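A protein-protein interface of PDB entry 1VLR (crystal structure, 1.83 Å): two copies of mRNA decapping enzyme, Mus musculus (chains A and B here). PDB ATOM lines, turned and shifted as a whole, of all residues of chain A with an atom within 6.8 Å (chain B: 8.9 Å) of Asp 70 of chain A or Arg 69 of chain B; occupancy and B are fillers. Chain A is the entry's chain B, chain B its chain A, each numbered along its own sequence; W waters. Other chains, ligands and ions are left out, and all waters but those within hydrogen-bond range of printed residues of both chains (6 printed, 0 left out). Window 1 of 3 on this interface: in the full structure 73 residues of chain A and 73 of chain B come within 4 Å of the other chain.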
ATOM      1  N   ARG A  65      13.198   6.938 -25.651  1.00  0.00           N
ATOM      2  CA  ARG A  65      13.151   8.386 -25.490  1.00  0.00           C
ATOM      3  C   ARG A  65      14.519   8.869 -25.052  1.00  0.00           C
ATOM      4  O   ARG A  65      15.215   8.192 -24.332  1.00  0.00           O
ATOM      5  CB  ARG A  65      12.105   8.773 -24.445  1.00  0.00           C
ATOM      6  CG  ARG A  65      11.924  10.275 -24.380  1.00  0.00           C
ATOM      7  CD  ARG A  65      10.705  10.746 -23.646  1.00  0.00           C
ATOM      8  NE  ARG A  65      10.838  10.800 -22.202  1.00  0.00           N
ATOM      9  CZ  ARG A  65      11.502  11.732 -21.524  1.00  0.00           C
ATOM     10  NH1 ARG A  65      12.206  12.678 -22.146  1.00  0.00           N
ATOM     11  NH2 ARG A  65      11.465  11.707 -20.201  1.00  0.00           N
ATOM     12  N   SER A  67      16.574  12.813 -24.030  1.00  0.00           N
ATOM     13  CA  SER A  67      16.479  14.257 -23.940  1.00  0.00           C
ATOM     14  C   SER A  67      17.838  14.812 -23.645  1.00  0.00           C
ATOM     15  O   SER A  67      18.442  14.556 -22.610  1.00  0.00           O
ATOM     16  CB  SER A  67      15.459  14.688 -22.874  1.00  0.00           C
ATOM     17  OG  SER A  67      15.448  16.106 -22.763  1.00  0.00           O
ATOM     18  N   ALA A  68      18.318  15.616 -24.570  1.00  0.00           N
ATOM     19  CA  ALA A  68      19.513  16.379 -24.360  1.00  0.00           C
ATOM     20  C   ALA A  68      19.287  17.497 -23.353  1.00  0.00           C
ATOM     21  O   ALA A  68      20.182  17.863 -22.606  1.00  0.00           O
ATOM     22  CB  ALA A  68      19.997  16.955 -25.709  1.00  0.00           C
ATOM     23  N   ARG A  69      18.078  18.045 -23.315  1.00  0.00           N
ATOM     24  CA  ARG A  69      17.769  19.062 -22.352  1.00  0.00           C
ATOM     25  C   ARG A  69      17.868  18.508 -20.925  1.00  0.00           C
ATOM     26  O   ARG A  69      18.511  19.111 -20.024  1.00  0.00           O
ATOM     27  CB  ARG A  69      16.373  19.626 -22.678  1.00  0.00           C
ATOM     28  CG  ARG A  69      16.024  20.844 -21.896  1.00  0.00           C
ATOM     29  CD  ARG A  69      14.570  21.205 -21.924  1.00  0.00           C
ATOM     30  NE  ARG A  69      13.772  20.251 -21.172  1.00  0.00           N
ATOM     31  CZ  ARG A  69      12.447  20.220 -21.183  1.00  0.00           C
ATOM     32  NH1 ARG A  69      11.768  21.080 -21.923  1.00  0.00           N
ATOM     33  NH2 ARG A  69      11.796  19.330 -20.441  1.00  0.00           N
ATOM     34  N   ASP A  70      17.245  17.348 -20.712  1.00  0.00           N
ATOM     35  CA  ASP A  70      17.092  16.754 -19.407  1.00  0.00           C
ATOM     36  C   ASP A  70      18.190  15.728 -19.034  1.00  0.00           C
ATOM     37  O   ASP A  70      18.299  15.323 -17.881  1.00  0.00           O
ATOM     38  CB  ASP A  70      15.733  16.117 -19.353  1.00  0.00           C
ATOM     39  CG  ASP A  70      14.596  17.161 -19.480  1.00  0.00           C
ATOM     40  OD1 ASP A  70      14.847  18.384 -19.480  1.00  0.00           O
ATOM     41  OD2 ASP A  70      13.438  16.823 -19.540  1.00  0.00           O
ATOM     42  N   LYS A  71      19.025  15.379 -20.009  1.00  0.00           N
ATOM     43  CA  LYS A  71      20.149  14.472 -19.832  1.00  0.00           C
ATOM     44  C   LYS A  71      19.685  13.133 -19.322  1.00  0.00           C
ATOM     45  O   LYS A  71      20.126  12.629 -18.294  1.00  0.00           O
ATOM     46  CB  LYS A  71      21.247  15.075 -18.954  1.00  0.00           C
ATOM     47  CG  LYS A  71      21.971  16.248 -19.688  1.00  0.00           C
ATOM     48  CD  LYS A  71      21.331  17.539 -19.390  1.00  0.00           C
ATOM     49  CE  LYS A  71      22.003  18.686 -20.102  1.00  0.00           C
ATOM     50  NZ  LYS A  71      21.058  19.820 -20.056  1.00  0.00           N
ATOM     51  N   ILE A  72      18.792  12.549 -20.102  1.00  0.00           N
ATOM     52  CA  ILE A  72      18.211  11.244 -19.769  1.00  0.00           C
ATOM     53  C   ILE A  72      18.060  10.460 -21.053  1.00  0.00           C
ATOM     54  O   ILE A  72      17.822  11.015 -22.130  1.00  0.00           O
ATOM     55  CB  ILE A  72      16.851  11.426 -19.026  1.00  0.00           C
ATOM     56  CG1 ILE A  72      16.365  10.088 -18.418  1.00  0.00           C
ATOM     57  CG2 ILE A  72      15.801  12.109 -19.975  1.00  0.00           C
ATOM     58  CD1 ILE A  72      15.327  10.230 -17.269  1.00  0.00           C
ATOM     59  N   GLU A  96      20.212   8.480 -16.248  1.00  0.00           N
ATOM     60  CA  GLU A  96      19.918   9.883 -16.009  1.00  0.00           C
ATOM     61  C   GLU A  96      21.083  10.579 -15.274  1.00  0.00           C
ATOM     62  O   GLU A  96      21.524  10.120 -14.225  1.00  0.00           O
ATOM     63  CB  GLU A  96      18.669  10.029 -15.155  1.00  0.00           C
ATOM     64  CG  GLU A  96      18.247  11.515 -15.024  1.00  0.00           C
ATOM     65  CD  GLU A  96      16.939  11.765 -14.257  1.00  0.00           C
ATOM     66  OE1 GLU A  96      16.488  12.956 -14.324  1.00  0.00           O
ATOM     67  OE2 GLU A  96      16.389  10.802 -13.645  1.00  0.00           O
ATOM     68  N   LYS A  97      21.599  11.663 -15.848  1.00  0.00           N
ATOM     69  CA  LYS A  97      22.599  12.467 -15.141  1.00  0.00           C
ATOM     70  C   LYS A  97      21.895  13.084 -13.949  1.00  0.00           C
ATOM     71  O   LYS A  97      20.729  13.435 -14.028  1.00  0.00           O
ATOM     72  CB  LYS A  97      23.205  13.552 -16.055  1.00  0.00           C
ATOM     73  CG  LYS A  97      23.945  13.047 -17.367  1.00  0.00           C
ATOM     74  CD  LYS A  97      25.135  12.176 -16.994  1.00  0.00           C
ATOM     75  CE  LYS A  97      25.979  11.693 -18.176  1.00  0.00           C
ATOM     76  NZ  LYS A  97      26.694  12.746 -18.924  1.00  0.00           N
ATOM     77  N   PRO A  99      21.210  15.968 -10.952  1.00  0.00           N
ATOM     78  CA  PRO A  99      21.373  17.389 -10.699  1.00  0.00           C
ATOM     79  C   PRO A  99      22.586  17.686  -9.849  1.00  0.00           C
ATOM     80  O   PRO A  99      23.046  16.824  -9.064  1.00  0.00           O
ATOM     81  CB  PRO A  99      20.140  17.762  -9.869  1.00  0.00           C
ATOM     82  CG  PRO A  99      19.172  16.652 -10.037  1.00  0.00           C
ATOM     83  CD  PRO A  99      19.968  15.447 -10.361  1.00  0.00           C
ATOM     84  N   PHE A 296       8.322  28.120 -13.067  1.00  0.00           N
ATOM     85  CA  PHE A 296       8.280  26.702 -13.151  1.00  0.00           C
ATOM     86  C   PHE A 296       7.589  26.423 -14.508  1.00  0.00           C
ATOM     87  O   PHE A 296       6.418  26.794 -14.699  1.00  0.00           O
ATOM     88  CB  PHE A 296       7.453  26.175 -11.977  1.00  0.00           C
ATOM     89  CG  PHE A 296       7.247  24.693 -11.937  1.00  0.00           C
ATOM     90  CD1 PHE A 296       8.227  23.796 -12.360  1.00  0.00           C
ATOM     91  CD2 PHE A 296       6.069  24.179 -11.427  1.00  0.00           C
ATOM     92  CE1 PHE A 296       7.981  22.455 -12.320  1.00  0.00           C
ATOM     93  CE2 PHE A 296       5.843  22.829 -11.351  1.00  0.00           C
ATOM     94  CZ  PHE A 296       6.790  21.964 -11.798  1.00  0.00           C
ATOM     95  N   GLU A 297       8.287  25.786 -15.437  1.00  0.00           N
ATOM     96  CA  GLU A 297       7.619  25.266 -16.639  1.00  0.00           C
ATOM     97  C   GLU A 297       6.766  24.065 -16.271  1.00  0.00           C
ATOM     98  O   GLU A 297       7.081  22.895 -16.550  1.00  0.00           O
ATOM     99  CB  GLU A 297       8.596  24.960 -17.752  1.00  0.00           C
ATOM    100  CG  GLU A 297       9.178  26.247 -18.259  1.00  0.00           C
ATOM    101  CD  GLU A 297      10.296  26.055 -19.243  1.00  0.00           C
ATOM    102  OE1 GLU A 297      10.525  24.897 -19.719  1.00  0.00           O
ATOM    103  OE2 GLU A 297      10.916  27.104 -19.553  1.00  0.00           O
ATOM    104  N   ALA A 298       5.638  24.386 -15.656  1.00  0.00           N
ATOM    105  CA  ALA A 298       4.798  23.397 -15.008  1.00  0.00           C
ATOM    106  C   ALA A 298       4.152  22.446 -16.035  1.00  0.00           C
ATOM    107  O   ALA A 298       4.158  22.736 -17.248  1.00  0.00           O
ATOM    108  CB  ALA A 298       3.727  24.109 -14.175  1.00  0.00           C
ATOM    109  N   GLU B  66      19.866  27.794 -11.059  1.00  0.00           N
ATOM    110  CA  GLU B  66      20.049  26.345 -11.196  1.00  0.00           C
ATOM    111  C   GLU B  66      18.779  25.632 -11.651  1.00  0.00           C
ATOM    112  O   GLU B  66      17.668  26.161 -11.511  1.00  0.00           O
ATOM    113  CB  GLU B  66      20.613  25.720  -9.932  1.00  0.00           C
ATOM    114  CG  GLU B  66      19.605  25.241  -8.934  1.00  0.00           C
ATOM    115  CD  GLU B  66      20.214  24.851  -7.629  1.00  0.00           C
ATOM    116  OE1 GLU B  66      20.661  23.687  -7.473  1.00  0.00           O
ATOM    117  OE2 GLU B  66      20.178  25.697  -6.723  1.00  0.00           O
ATOM    118  N   SER B  67      18.980  24.473 -12.272  1.00  0.00           N
ATOM    119  CA  SER B  67      17.868  23.694 -12.815  1.00  0.00           C
ATOM    120  C   SER B  67      18.224  22.262 -12.570  1.00  0.00           C
ATOM    121  O   SER B  67      19.152  21.740 -13.161  1.00  0.00           O
ATOM    122  CB  SER B  67      17.617  23.992 -14.298  1.00  0.00           C
ATOM    123  OG  SER B  67      16.614  23.148 -14.874  1.00  0.00           O
ATOM    124  N   ALA B  68      17.521  21.669 -11.618  1.00  0.00           N
ATOM    125  CA  ALA B  68      17.516  20.235 -11.444  1.00  0.00           C
ATOM    126  C   ALA B  68      17.052  19.514 -12.707  1.00  0.00           C
ATOM    127  O   ALA B  68      17.557  18.459 -12.989  1.00  0.00           O
ATOM    128  CB  ALA B  68      16.639  19.847 -10.253  1.00  0.00           C
ATOM    129  N   ARG B  69      16.122  20.096 -13.467  1.00  0.00           N
ATOM    130  CA  ARG B  69      15.615  19.476 -14.676  1.00  0.00           C
ATOM    131  C   ARG B  69      16.669  19.348 -15.749  1.00  0.00           C
ATOM    132  O   ARG B  69      16.766  18.337 -16.404  1.00  0.00           O
ATOM    133  CB  ARG B  69      14.465  20.286 -15.256  1.00  0.00           C
ATOM    134  CG  ARG B  69      13.766  19.623 -16.387  1.00  0.00           C
ATOM    135  CD  ARG B  69      12.705  20.501 -16.994  1.00  0.00           C
ATOM    136  NE  ARG B  69      13.350  21.530 -17.793  1.00  0.00           N
ATOM    137  CZ  ARG B  69      12.741  22.493 -18.457  1.00  0.00           C
ATOM    138  NH1 ARG B  69      11.435  22.613 -18.403  1.00  0.00           N
ATOM    139  NH2 ARG B  69      13.463  23.349 -19.179  1.00  0.00           N
ATOM    140  N   ASP B  70      17.389  20.430 -15.957  1.00  0.00           N
ATOM    141  CA  ASP B  70      18.304  20.572 -17.048  1.00  0.00           C
ATOM    142  C   ASP B  70      19.733  20.171 -16.624  1.00  0.00           C
ATOM    143  O   ASP B  70      20.643  20.205 -17.456  1.00  0.00           O
ATOM    144  CB  ASP B  70      18.310  22.002 -17.534  1.00  0.00           C
ATOM    145  CG  ASP B  70      17.002  22.409 -18.196  1.00  0.00           C
ATOM    146  OD1 ASP B  70      16.052  21.612 -18.296  1.00  0.00           O
ATOM    147  OD2 ASP B  70      16.856  23.516 -18.667  1.00  0.00           O
ATOM    148  N   LYS B  71      19.921  19.886 -15.335  1.00  0.00           N
ATOM    149  CA  LYS B  71      21.205  19.400 -14.781  1.00  0.00           C
ATOM    150  C   LYS B  71      22.267  20.481 -15.042  1.00  0.00           C
ATOM    151  O   LYS B  71      23.303  20.232 -15.624  1.00  0.00           O
ATOM    152  CB  LYS B  71      21.586  18.051 -15.397  1.00  0.00           C
ATOM    153  CG  LYS B  71      20.378  17.066 -15.544  1.00  0.00           C
ATOM    154  CD  LYS B  71      19.902  16.654 -14.226  1.00  0.00           C
ATOM    155  CE  LYS B  71      18.523  16.003 -14.293  1.00  0.00           C
ATOM    156  NZ  LYS B  71      18.403  14.965 -15.260  1.00  0.00           N
ATOM    157  N   ILE B  72      21.956  21.711 -14.621  1.00  0.00           N
ATOM    158  CA  ILE B  72      22.833  22.845 -14.859  1.00  0.00           C
ATOM    159  C   ILE B  72      22.838  23.734 -13.633  1.00  0.00           C
ATOM    160  O   ILE B  72      21.847  23.799 -12.894  1.00  0.00           O
ATOM    161  CB  ILE B  72      22.431  23.570 -16.181  1.00  0.00           C
ATOM    162  CG1 ILE B  72      23.464  24.618 -16.574  1.00  0.00           C
ATOM    163  CG2 ILE B  72      21.083  24.231 -16.061  1.00  0.00           C
ATOM    164  CD1 ILE B  72      23.326  25.113 -17.896  1.00  0.00           C
ATOM    165  N   GLU B  96      27.361  22.053 -16.482  1.00  0.00           N
ATOM    166  CA  GLU B  96      26.234  21.388 -17.123  1.00  0.00           C
ATOM    167  C   GLU B  96      26.604  19.939 -17.382  1.00  0.00           C
ATOM    168  O   GLU B  96      27.639  19.666 -17.972  1.00  0.00           O
ATOM    169  CB  GLU B  96      25.875  22.057 -18.450  1.00  0.00           C
ATOM    170  CG  GLU B  96      24.483  21.628 -18.940  1.00  0.00           C
ATOM    171  CD  GLU B  96      24.042  22.284 -20.244  1.00  0.00           C
ATOM    172  OE1 GLU B  96      24.809  23.138 -20.773  1.00  0.00           O
ATOM    173  OE2 GLU B  96      22.935  21.918 -20.764  1.00  0.00           O
ATOM    174  N   LYS B  97      25.805  19.005 -16.874  1.00  0.00           N
ATOM    175  CA  LYS B  97      26.028  17.610 -17.158  1.00  0.00           C
ATOM    176  C   LYS B  97      25.799  17.457 -18.643  1.00  0.00           C
ATOM    177  O   LYS B  97      25.040  18.230 -19.235  1.00  0.00           O
ATOM    178  CB  LYS B  97      25.108  16.685 -16.369  1.00  0.00           C
ATOM    179  CG  LYS B  97      25.180  16.811 -14.881  1.00  0.00           C
ATOM    180  CD  LYS B  97      26.398  16.139 -14.321  1.00  0.00           C
ATOM    181  CE  LYS B  97      26.405  16.232 -12.804  1.00  0.00           C
ATOM    182  NZ  LYS B  97      25.572  15.175 -12.065  1.00  0.00           N
ATOM    183  N   THR B  98      26.461  16.464 -19.240  1.00  0.00           N
ATOM    184  CA  THR B  98      26.365  16.236 -20.657  1.00  0.00           C
ATOM    185  C   THR B  98      25.245  15.284 -21.011  1.00  0.00           C
ATOM    186  O   THR B  98      24.917  14.365 -20.241  1.00  0.00           O
ATOM    187  CB  THR B  98      27.689  15.706 -21.222  1.00  0.00           C
ATOM    188  OG1 THR B  98      28.181  14.640 -20.383  1.00  0.00           O
ATOM    189  CG2 THR B  98      28.746  16.844 -21.146  1.00  0.00           C
ATOM    190  N   PRO B  99      24.686  15.488 -22.192  1.00  0.00           N
ATOM    191  CA  PRO B  99      23.712  14.552 -22.706  1.00  0.00           C
ATOM    192  C   PRO B  99      24.354  13.214 -22.996  1.00  0.00           C
ATOM    193  O   PRO B  99      25.536  13.129 -23.285  1.00  0.00           O
ATOM    194  CB  PRO B  99      23.235  15.185 -23.994  1.00  0.00           C
ATOM    195  CG  PRO B  99      23.721  16.552 -24.011  1.00  0.00           C
ATOM    196  CD  PRO B  99      24.921  16.605 -23.113  1.00  0.00           C
ATOM    197  N   PHE B 100      23.554  12.180 -23.017  1.00  0.00           N
ATOM    198  CA  PHE B 100      24.068  10.861 -23.381  1.00  0.00           C
ATOM    199  C   PHE B 100      24.257  10.626 -24.881  1.00  0.00           C
ATOM    200  O   PHE B 100      23.482  11.103 -25.721  1.00  0.00           O
ATOM    201  CB  PHE B 100      23.087   9.815 -22.873  1.00  0.00           C
ATOM    202  CG  PHE B 100      23.094   9.692 -21.433  1.00  0.00           C
ATOM    203  CD1 PHE B 100      24.138   9.054 -20.811  1.00  0.00           C
ATOM    204  CD2 PHE B 100      22.111  10.274 -20.665  1.00  0.00           C
ATOM    205  CE1 PHE B 100      24.179   8.943 -19.430  1.00  0.00           C
ATOM    206  CE2 PHE B 100      22.155  10.173 -19.291  1.00  0.00           C
ATOM    207  CZ  PHE B 100      23.202   9.507 -18.674  1.00  0.00           C
ATOM    208  N   GLU B 297       9.387  21.924 -27.009  1.00  0.00           N
ATOM    209  CA  GLU B 297       8.938  22.963 -26.052  1.00  0.00           C
ATOM    210  C   GLU B 297       9.712  24.247 -26.313  1.00  0.00           C
ATOM    211  O   GLU B 297      10.615  24.636 -25.559  1.00  0.00           O
ATOM    212  CB  GLU B 297       9.073  22.479 -24.608  1.00  0.00           C
ATOM    213  CG  GLU B 297       8.195  21.258 -24.375  1.00  0.00           C
ATOM    214  CD  GLU B 297       8.095  20.773 -22.942  1.00  0.00           C
ATOM    215  OE1 GLU B 297       8.816  21.289 -22.040  1.00  0.00           O
ATOM    216  OE2 GLU B 297       7.262  19.845 -22.717  1.00  0.00           O
HETATM  217  O   HOH W   1      27.324  11.654 -21.522  1.00  0.00           O
HETATM  218  O   HOH W   2       8.585  23.625 -20.902  1.00  0.00           O
HETATM  219  O   HOH W   3      28.026  14.627 -17.232  1.00  0.00           O
HETATM  220  O   HOH W   4      26.430  16.023  -9.453  1.00  0.00           O
HETATM  221  O   HOH W   5      20.730  12.619 -23.128  1.00  0.00           O
HETATM  222  O   HOH W   6       9.178  20.971 -18.151  1.00  0.00           O
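Ala 68 of chain A touches Pro 99 of chain B, and with the chains exchanged Pro 99 of chain A touches Ala 68 of chain B.
Arg 69 of chain A touches Glu 297 of chain B, and with the chains exchanged Glu 297 of chain A touches Arg 69 of chain B.
Lys 71 of chain B touches its own counterpart, Lys 71 of chain A.
Lys 71 of chain A touches Glu 96 of chain B, and with the chains exchanged Glu 96 of chain A touches Lys 71 of chain B.
Of the 23 pairs that touch across the chains among the printed residues, 18 have their exchanged pair printed and touching as well.
Water W2 bridges the side-chain carboxylate (OE1) of Glu 297 of chain A (2.6 Å) and the side-chain carboxylate (OE1) of Glu 297 of chain B (2.6 Å).
Water W6 lies within hydrogen-bond range of NH1 of Arg 69 of chain B and O of Glu 297 of chain A.
Water W3 lies within hydrogen-bond range of NZ of Lys 97 of chain A (2.9 Å) and N of Thr 98 of chain B (3.1 Å).
Water W5 lies within hydrogen-bond range of N of Phe 100 of chain B, O of Ser 67 of chain A and O of Ile 72 of chain A.
Water W4 bridges NZ of Lys 97 of chain B (2.9 Å) and O of Pro 99 of chain A (3.5 Å).
Water W1 lies within hydrogen-bond range of the side-chain amino group (NZ) of Lys 97 of chain A (2.9 Å), the backbone carbonyl oxygen (O) of Pro 99 of chain B (2.9 Å) and the side-chain hydroxyl (OG1) of Thr 98 of chain B (3.3 Å).
OD1 of Asp 70 of chain A is in salt-bridge range of NE of Arg 69 of chain B, 3.9 Å away.
OE1 of Glu 297 of chain A lies within salt-bridge range of NH1 of Arg 69 of chain B, at 2.8 Å.
OD1 of Asp 70 of chain B is in salt-bridge range of NE of Arg 69 of chain A (3.9 Å).
O of Asp 70 of chain B lies within hydrogen-bond range of NZ of Lys 71 of chain A, 2.7 Å away.
The backbone carbonyl oxygen of Asp 70 of chain A sits at hydrogen-bond distance from the side-chain amino group of Lys 71 of chain B, 2.6 Å away.
The side-chain amino group (NZ) of Lys 71 of chain B is in salt-bridge range of the side-chain carboxylate (OE1) of Glu 96 of chain A (2.9 Å).
NZ of Lys 71 of chain B lies within hydrogen-bond range of O of Lys 97 of chain A (3.0 Å).
The side-chain carboxylate of Glu 96 of chain B is in salt-bridge range of the side-chain amino group of Lys 71 of chain A, 2.9 Å away.
The side-chain amino group of Lys 97 of chain A sits at hydrogen-bond distance from the backbone carbonyl oxygen of Thr 98 of chain B, 2.7 Å away.
OE1 of Glu 297 of chain B is in salt-bridge range of NH1 of Arg 69 of chain A (3.0 Å).
Asp 70 of chain A touches just these residues of chain B: Arg 69 (3.4 Å), Asp 70 (3.6 Å) and Lys 71 (2.6 Å).
Arg 69 of chain B touches three residues of chain A.
Arg 69 of chain A touches just these residues of chain B: Arg 69, Asp 70 and Glu 297.
Of the printed residues of chain B, Glu 297 of chain A touches Arg 69.
Of the printed residues of chain B, Lys 97 of chain A touches Lys 71 (3.0 Å), Lys 97 (3.7 Å), Thr 98 (2.7 Å) and Phe 100 (3.5 Å).
Phe 296 of chain A touches none of the printed residues of chain B.
Ile 72 of chain A touches none of the printed residues of chain B.
The nearest residue of chain A that does not touch Arg 69 of chain B is Lys 71 of chain A (5.2 Å).
Among the printed residues, merely in contact across the chains: Lys 71 of chain A with Lys 97 of chain B, Lys 71 of chain A with Phe 100 of chain B, Lys 97 of chain A with Phe 100 of chain B, Lys 71 of chain A with Thr 98 of chain B, Arg 69 of chain A with Arg 69 of chain B, Pro 99 of chain A with Lys 71 of chain B, Asp 70 of chain A with Asp 70 of chain B, Lys 97 of chain A with Lys 97 of chain B, Lys 71 of chain A with Pro 99 of chain B, Pro 99 of chain A with Ala 68 of chain B, Ala 68 of chain A with Pro 99 of chain B, Glu 96 of chain A with Phe 100 of chain B and Lys 71 of chain A with Lys 71 of chain B.
OG of Ser 67 of chain B sits close to N of Arg 69 of chain B, 3.4 Å away.
The side-chain hydroxyl (OG) of Ser 67 of chain B lies within hydrogen-bond range of the backbone NH (N) of Asp 70 of chain B (3.0 Å).
NE of Arg 69 of chain B is in salt-bridge range of OD1 of Asp 70 of chain B (2.7 Å).
The backbone NH of Lys 97 of chain B is in hydrogen-bond range of the backbone carbonyl oxygen of Lys 71 of chain B (3.1 Å).
O of Ala 68 of chain A sits close to NZ of Lys 71 of chain A (3.3 Å).
O of Lys 71 of chain A sits at hydrogen-bond distance from N of Lys 97 of chain A (3.0 Å).
Hydrophobic or aromatic side chains of chain B that line the printed part of chain A: Pro 99 and Phe 100.
Of the 13 printed residues of chain A, 8 touch a printed residue of chain B.
Printed residues of chain A that touch a printed residue of chain B: Ala 68, Arg 69, Asp 70, Lys 71, Glu 96, Lys 97, Pro 99 and Glu 297.
Hydrophobic or aromatic side chains of chain A within 4 Å of the printed part of chain B: Pro 99.
Along chain A the printed residues that touch a printed residue of chain B span positions 68 to 297.
Among the printed residues, Asp or Glu carboxylates within 4 Å of a Lys or Arg side-chain nitrogen of the other chain: Arg 69 of chain A with Asp 70 of chain B, Arg 69 of chain A with Glu 297 of chain B, Asp 70 of chain A with Arg 69 of chain B, Lys 71 of chain A with Glu 96 of chain B, Glu 96 of chain A with Lys 71 of chain B and Glu 297 of chain A with Arg 69 of chain B.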
